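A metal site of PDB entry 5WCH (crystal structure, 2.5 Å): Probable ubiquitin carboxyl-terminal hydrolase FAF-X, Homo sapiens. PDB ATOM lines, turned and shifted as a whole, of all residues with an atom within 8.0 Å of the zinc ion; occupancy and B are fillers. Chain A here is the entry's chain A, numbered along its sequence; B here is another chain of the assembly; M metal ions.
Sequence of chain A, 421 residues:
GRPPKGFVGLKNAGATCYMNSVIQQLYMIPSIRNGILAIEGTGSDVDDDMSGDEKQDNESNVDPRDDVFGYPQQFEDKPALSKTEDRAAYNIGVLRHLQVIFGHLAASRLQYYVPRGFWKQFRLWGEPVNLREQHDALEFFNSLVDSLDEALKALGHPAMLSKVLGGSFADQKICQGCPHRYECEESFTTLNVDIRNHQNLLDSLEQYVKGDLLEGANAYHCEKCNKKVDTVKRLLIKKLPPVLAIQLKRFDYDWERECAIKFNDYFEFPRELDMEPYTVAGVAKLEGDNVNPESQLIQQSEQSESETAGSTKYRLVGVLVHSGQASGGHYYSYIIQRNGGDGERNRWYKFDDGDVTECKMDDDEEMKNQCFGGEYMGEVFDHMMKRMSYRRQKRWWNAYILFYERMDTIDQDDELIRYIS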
ATOM      1  N   CYS A 175      26.871  30.985   4.626  1.00  0.00           N
ATOM      2  CA  CYS A 175      25.711  30.574   3.864  1.00  0.00           C
ATOM      3  C   CYS A 175      25.558  31.506   2.663  1.00  0.00           C
ATOM      4  O   CYS A 175      25.655  32.726   2.797  1.00  0.00           O
ATOM      5  CB  CYS A 175      24.461  30.572   4.729  1.00  0.00           C
ATOM      6  SG  CYS A 175      24.644  29.572   6.243  1.00  0.00           S
ATOM      7  N   GLY A 177      22.891  30.973   0.275  1.00  0.00           N
ATOM      8  CA  GLY A 177      21.446  31.110   0.041  1.00  0.00           C
ATOM      9  C   GLY A 177      20.658  31.719   1.191  1.00  0.00           C
ATOM     10  O   GLY A 177      19.440  31.583   1.210  1.00  0.00           O
ATOM     11  N   CYS A 178      21.343  32.354   2.152  1.00  0.00           N
ATOM     12  CA  CYS A 178      20.709  33.033   3.283  1.00  0.00           C
ATOM     13  C   CYS A 178      21.744  33.961   3.941  1.00  0.00           C
ATOM     14  O   CYS A 178      22.937  33.785   3.745  1.00  0.00           O
ATOM     15  CB  CYS A 178      20.142  32.020   4.290  1.00  0.00           C
ATOM     16  SG  CYS A 178      21.294  31.283   5.482  1.00  0.00           S
ATOM     17  N   PRO A 179      21.296  34.941   4.743  1.00  0.00           N
ATOM     18  CA  PRO A 179      22.251  35.905   5.263  1.00  0.00           C
ATOM     19  C   PRO A 179      23.086  35.422   6.449  1.00  0.00           C
ATOM     20  O   PRO A 179      23.853  36.206   6.989  1.00  0.00           O
ATOM     21  CB  PRO A 179      21.328  37.041   5.732  1.00  0.00           C
ATOM     22  CG  PRO A 179      20.161  36.306   6.261  1.00  0.00           C
ATOM     23  CD  PRO A 179      19.971  35.122   5.355  1.00  0.00           C
ATOM     24  N   HIS A 180      22.944  34.176   6.866  1.00  0.00           N
ATOM     25  CA  HIS A 180      23.626  33.725   8.070  1.00  0.00           C
ATOM     26  C   HIS A 180      25.060  33.283   7.864  1.00  0.00           C
ATOM     27  O   HIS A 180      25.468  32.844   6.772  1.00  0.00           O
ATOM     28  CB  HIS A 180      22.838  32.617   8.747  1.00  0.00           C
ATOM     29  CG  HIS A 180      21.565  33.106   9.356  1.00  0.00           C
ATOM     30  ND1 HIS A 180      20.335  32.883   8.783  1.00  0.00           N
ATOM     31  CD2 HIS A 180      21.345  33.874  10.441  1.00  0.00           C
ATOM     32  CE1 HIS A 180      19.399  33.470   9.508  1.00  0.00           C
ATOM     33  NE2 HIS A 180      19.990  34.076  10.522  1.00  0.00           N
ATOM     34  N   ARG A 181      25.793  33.384   8.956  1.00  0.00           N
ATOM     35  CA  ARG A 181      27.196  33.046   9.008  1.00  0.00           C
ATOM     36  C   ARG A 181      27.440  32.459  10.399  1.00  0.00           C
ATOM     37  O   ARG A 181      26.873  32.936  11.366  1.00  0.00           O
ATOM     38  CB  ARG A 181      27.993  34.323   8.760  1.00  0.00           C
ATOM     39  CG  ARG A 181      29.480  34.155   8.794  1.00  0.00           C
ATOM     40  CD  ARG A 181      30.165  35.258   8.013  1.00  0.00           C
ATOM     41  NE  ARG A 181      31.607  35.315   8.290  1.00  0.00           N
ATOM     42  CZ  ARG A 181      32.459  36.139   7.690  1.00  0.00           C
ATOM     43  NH1 ARG A 181      32.037  36.999   6.748  1.00  0.00           N
ATOM     44  NH2 ARG A 181      33.736  36.113   8.025  1.00  0.00           N
ATOM     45  N   TYR A 182      28.225  31.391  10.477  1.00  0.00           N
ATOM     46  CA  TYR A 182      28.495  30.702  11.738  1.00  0.00           C
ATOM     47  C   TYR A 182      29.982  30.498  11.900  1.00  0.00           C
ATOM     48  O   TYR A 182      30.660  30.058  10.987  1.00  0.00           O
ATOM     49  CB  TYR A 182      27.792  29.339  11.792  1.00  0.00           C
ATOM     50  CG  TYR A 182      26.289  29.417  11.652  1.00  0.00           C
ATOM     51  CD1 TYR A 182      25.478  29.656  12.758  1.00  0.00           C
ATOM     52  CD2 TYR A 182      25.681  29.266  10.409  1.00  0.00           C
ATOM     53  CE1 TYR A 182      24.091  29.730  12.624  1.00  0.00           C
ATOM     54  CE2 TYR A 182      24.307  29.331  10.267  1.00  0.00           C
ATOM     55  CZ  TYR A 182      23.522  29.563  11.372  1.00  0.00           C
ATOM     56  OH  TYR A 182      22.169  29.628  11.202  1.00  0.00           O
ATOM     57  N   TYR A 220      24.384  22.409   3.838  1.00  0.00           N
ATOM     58  CA  TYR A 220      24.412  22.743   5.257  1.00  0.00           C
ATOM     59  C   TYR A 220      23.022  23.048   5.787  1.00  0.00           C
ATOM     60  O   TYR A 220      22.224  23.721   5.123  1.00  0.00           O
ATOM     61  CB  TYR A 220      25.289  23.970   5.451  1.00  0.00           C
ATOM     62  CG  TYR A 220      25.481  24.437   6.877  1.00  0.00           C
ATOM     63  CD1 TYR A 220      26.235  23.692   7.783  1.00  0.00           C
ATOM     64  CD2 TYR A 220      24.979  25.666   7.296  1.00  0.00           C
ATOM     65  CE1 TYR A 220      26.448  24.135   9.070  1.00  0.00           C
ATOM     66  CE2 TYR A 220      25.186  26.117   8.579  1.00  0.00           C
ATOM     67  CZ  TYR A 220      25.922  25.357   9.461  1.00  0.00           C
ATOM     68  OH  TYR A 220      26.124  25.814  10.740  1.00  0.00           O
ATOM     69  N   HIS A 221      22.762  22.609   7.011  1.00  0.00           N
ATOM     70  CA  HIS A 221      21.514  22.957   7.659  1.00  0.00           C
ATOM     71  C   HIS A 221      21.721  24.245   8.457  1.00  0.00           C
ATOM     72  O   HIS A 221      22.409  24.252   9.476  1.00  0.00           O
ATOM     73  CB  HIS A 221      20.989  21.821   8.548  1.00  0.00           C
ATOM     74  CG  HIS A 221      19.529  21.934   8.831  1.00  0.00           C
ATOM     75  ND1 HIS A 221      19.019  22.772   9.804  1.00  0.00           N
ATOM     76  CD2 HIS A 221      18.450  21.370   8.222  1.00  0.00           C
ATOM     77  CE1 HIS A 221      17.699  22.694   9.799  1.00  0.00           C
ATOM     78  NE2 HIS A 221      17.335  21.852   8.844  1.00  0.00           N
ATOM     79  N   CYS A 222      21.149  25.342   7.960  1.00  0.00           N
ATOM     80  CA  CYS A 222      21.059  26.574   8.730  1.00  0.00           C
ATOM     81  C   CYS A 222      19.975  26.380   9.760  1.00  0.00           C
ATOM     82  O   CYS A 222      18.828  26.095   9.396  1.00  0.00           O
ATOM     83  CB  CYS A 222      20.701  27.761   7.845  1.00  0.00           C
ATOM     84  SG  CYS A 222      20.441  29.279   8.773  1.00  0.00           S
ATOM     85  N   GLU A 223      20.329  26.528  11.029  1.00  0.00           N
ATOM     86  CA  GLU A 223      19.389  26.171  12.091  1.00  0.00           C
ATOM     87  C   GLU A 223      18.401  27.289  12.383  1.00  0.00           C
ATOM     88  O   GLU A 223      17.359  27.040  12.989  1.00  0.00           O
ATOM     89  CB  GLU A 223      20.120  25.651  13.351  1.00  0.00           C
ATOM     90  CG  GLU A 223      20.647  26.688  14.342  1.00  0.00           C
ATOM     91  CD  GLU A 223      20.882  26.091  15.730  1.00  0.00           C
ATOM     92  OE1 GLU A 223      20.812  26.855  16.726  1.00  0.00           O
ATOM     93  OE2 GLU A 223      21.120  24.864  15.844  1.00  0.00           O
ATOM     94  N   LYS A 224      18.710  28.507  11.956  1.00  0.00           N
ATOM     95  CA  LYS A 224      17.829  29.649  12.171  1.00  0.00           C
ATOM     96  C   LYS A 224      16.804  29.695  11.074  1.00  0.00           C
ATOM     97  O   LYS A 224      15.601  29.763  11.342  1.00  0.00           O
ATOM     98  CB  LYS A 224      18.631  30.934  12.209  1.00  0.00           C
ATOM     99  CG  LYS A 224      19.690  30.909  13.295  1.00  0.00           C
ATOM    100  CD  LYS A 224      20.002  32.284  13.842  1.00  0.00           C
ATOM    101  CE  LYS A 224      20.589  32.156  15.238  1.00  0.00           C
ATOM    102  NZ  LYS A 224      19.605  31.590  16.201  1.00  0.00           N
ATOM    103  N   CYS A 225      17.276  29.655   9.832  1.00  0.00           N
ATOM    104  CA  CYS A 225      16.395  29.544   8.686  1.00  0.00           C
ATOM    105  C   CYS A 225      15.625  28.207   8.683  1.00  0.00           C
ATOM    106  O   CYS A 225      14.565  28.120   8.088  1.00  0.00           O
ATOM    107  CB  CYS A 225      17.169  29.732   7.378  1.00  0.00           C
ATOM    108  SG  CYS A 225      17.732  31.431   7.082  1.00  0.00           S
ATOM    109  N   ASN A 226      16.155  27.175   9.341  1.00  0.00           N
ATOM    110  CA  ASN A 226      15.520  25.854   9.375  1.00  0.00           C
ATOM    111  C   ASN A 226      15.325  25.252   7.964  1.00  0.00           C
ATOM    112  O   ASN A 226      14.248  24.806   7.594  1.00  0.00           O
ATOM    113  CB  ASN A 226      14.196  25.878  10.170  1.00  0.00           C
ATOM    114  CG  ASN A 226      13.702  24.468  10.500  1.00  0.00           C
ATOM    115  OD1 ASN A 226      14.466  23.632  10.964  1.00  0.00           O
ATOM    116  ND2 ASN A 226      12.431  24.212  10.252  1.00  0.00           N
ATOM    117  N   LYS A 227      16.397  25.265   7.189  1.00  0.00           N
ATOM    118  CA  LYS A 227      16.415  24.664   5.875  1.00  0.00           C
ATOM    119  C   LYS A 227      17.839  24.340   5.480  1.00  0.00           C
ATOM    120  O   LYS A 227      18.770  24.804   6.118  1.00  0.00           O
ATOM    121  CB  LYS A 227      15.788  25.611   4.855  1.00  0.00           C
ATOM    122  CG  LYS A 227      16.448  26.978   4.794  1.00  0.00           C
ATOM    123  CD  LYS A 227      15.723  27.904   3.847  1.00  0.00           C
ATOM    124  CE  LYS A 227      16.608  29.070   3.463  1.00  0.00           C
ATOM    125  NZ  LYS A 227      15.918  29.995   2.535  1.00  0.00           N
ATOM    126  N   VAL A 229      20.841  24.929   3.007  1.00  0.00           N
ATOM    127  CA  VAL A 229      21.289  26.104   2.281  1.00  0.00           C
ATOM    128  C   VAL A 229      22.746  25.892   1.794  1.00  0.00           C
ATOM    129  O   VAL A 229      23.553  25.314   2.511  1.00  0.00           O
ATOM    130  CB  VAL A 229      21.120  27.366   3.157  1.00  0.00           C
ATOM    131  CG1 VAL A 229      22.017  27.328   4.387  1.00  0.00           C
ATOM    132  CG2 VAL A 229      21.385  28.629   2.374  1.00  0.00           C
ATOM    133  N   THR A 231      26.504  26.523   1.101  1.00  0.00           N
ATOM    134  CA  THR A 231      27.372  27.104   2.106  1.00  0.00           C
ATOM    135  C   THR A 231      28.860  26.768   1.886  1.00  0.00           C
ATOM    136  O   THR A 231      29.206  25.612   1.581  1.00  0.00           O
ATOM    137  CB  THR A 231      26.927  26.611   3.508  1.00  0.00           C
ATOM    138  OG1 THR A 231      25.573  27.023   3.746  1.00  0.00           O
ATOM    139  CG2 THR A 231      27.841  27.135   4.637  1.00  0.00           C
ATOM    140  N   TRP B 125      14.756  38.060   9.052  1.00  0.00           N
ATOM    141  CA  TRP B 125      16.163  38.157   8.671  1.00  0.00           C
ATOM    142  C   TRP B 125      16.394  39.428   7.875  1.00  0.00           C
ATOM    143  O   TRP B 125      16.774  39.395   6.696  1.00  0.00           O
ATOM    144  CB  TRP B 125      16.616  36.921   7.885  1.00  0.00           C
ATOM    145  CG  TRP B 125      16.078  35.651   8.434  1.00  0.00           C
ATOM    146  CD1 TRP B 125      15.334  34.724   7.769  1.00  0.00           C
ATOM    147  CD2 TRP B 125      16.223  35.168   9.777  1.00  0.00           C
ATOM    148  NE1 TRP B 125      15.015  33.691   8.604  1.00  0.00           N
ATOM    149  CE2 TRP B 125      15.543  33.932   9.845  1.00  0.00           C
ATOM    150  CE3 TRP B 125      16.858  35.646  10.919  1.00  0.00           C
ATOM    151  CZ2 TRP B 125      15.484  33.180  11.014  1.00  0.00           C
ATOM    152  CZ3 TRP B 125      16.799  34.895  12.088  1.00  0.00           C
ATOM    153  CH2 TRP B 125      16.103  33.684  12.126  1.00  0.00           C
ATOM    154  N   GLU B 139      11.036  28.997  11.543  1.00  0.00           N
ATOM    155  CA  GLU B 139      11.839  30.125  11.089  1.00  0.00           C
ATOM    156  C   GLU B 139      11.360  31.438  11.758  1.00  0.00           C
ATOM    157  O   GLU B 139      12.172  32.264  12.168  1.00  0.00           O
ATOM    158  CB  GLU B 139      11.771  30.205   9.566  1.00  0.00           C
ATOM    159  CG  GLU B 139      12.774  31.146   8.937  1.00  0.00           C
ATOM    160  CD  GLU B 139      13.002  30.914   7.443  1.00  0.00           C
ATOM    161  OE1 GLU B 139      12.572  29.869   6.871  1.00  0.00           O
ATOM    162  OE2 GLU B 139      13.630  31.802   6.824  1.00  0.00           O
HETATM  163 ZN    ZN M   1      20.027  31.099   7.467  1.00  0.00          ZN
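The backbone carbonyl oxygen of His 180 lies within hydrogen-bond range of the backbone NH of Cys 175 (3.2 Å). The side-chain hydroxyl (OH) of Tyr 182 sits close to the side-chain sulfur (SG) of Cys 222 (3.0 Å). The backbone NH (N) of Cys 222 lies within hydrogen-bond range of the backbone carbonyl oxygen (O) of Lys 227 (3.1 Å). SG of Cys 222 lies close to N of Lys 224, at 3.7 Å.
Of the 19 residues printed, 4 come within 4 Å of the zinc ion. The nearest printed residue that does not touch the zinc ion is Pro 179 (4.5 Å).
ND1 of His 180 binds the zinc ion, 2.2 Å away. The side-chain sulfur (SG) of Cys 222 is bound to the zinc ion. SG of Cys 225 is bound to the zinc ion (2.4 Å). The zinc ion is bound by SG of Cys 178.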
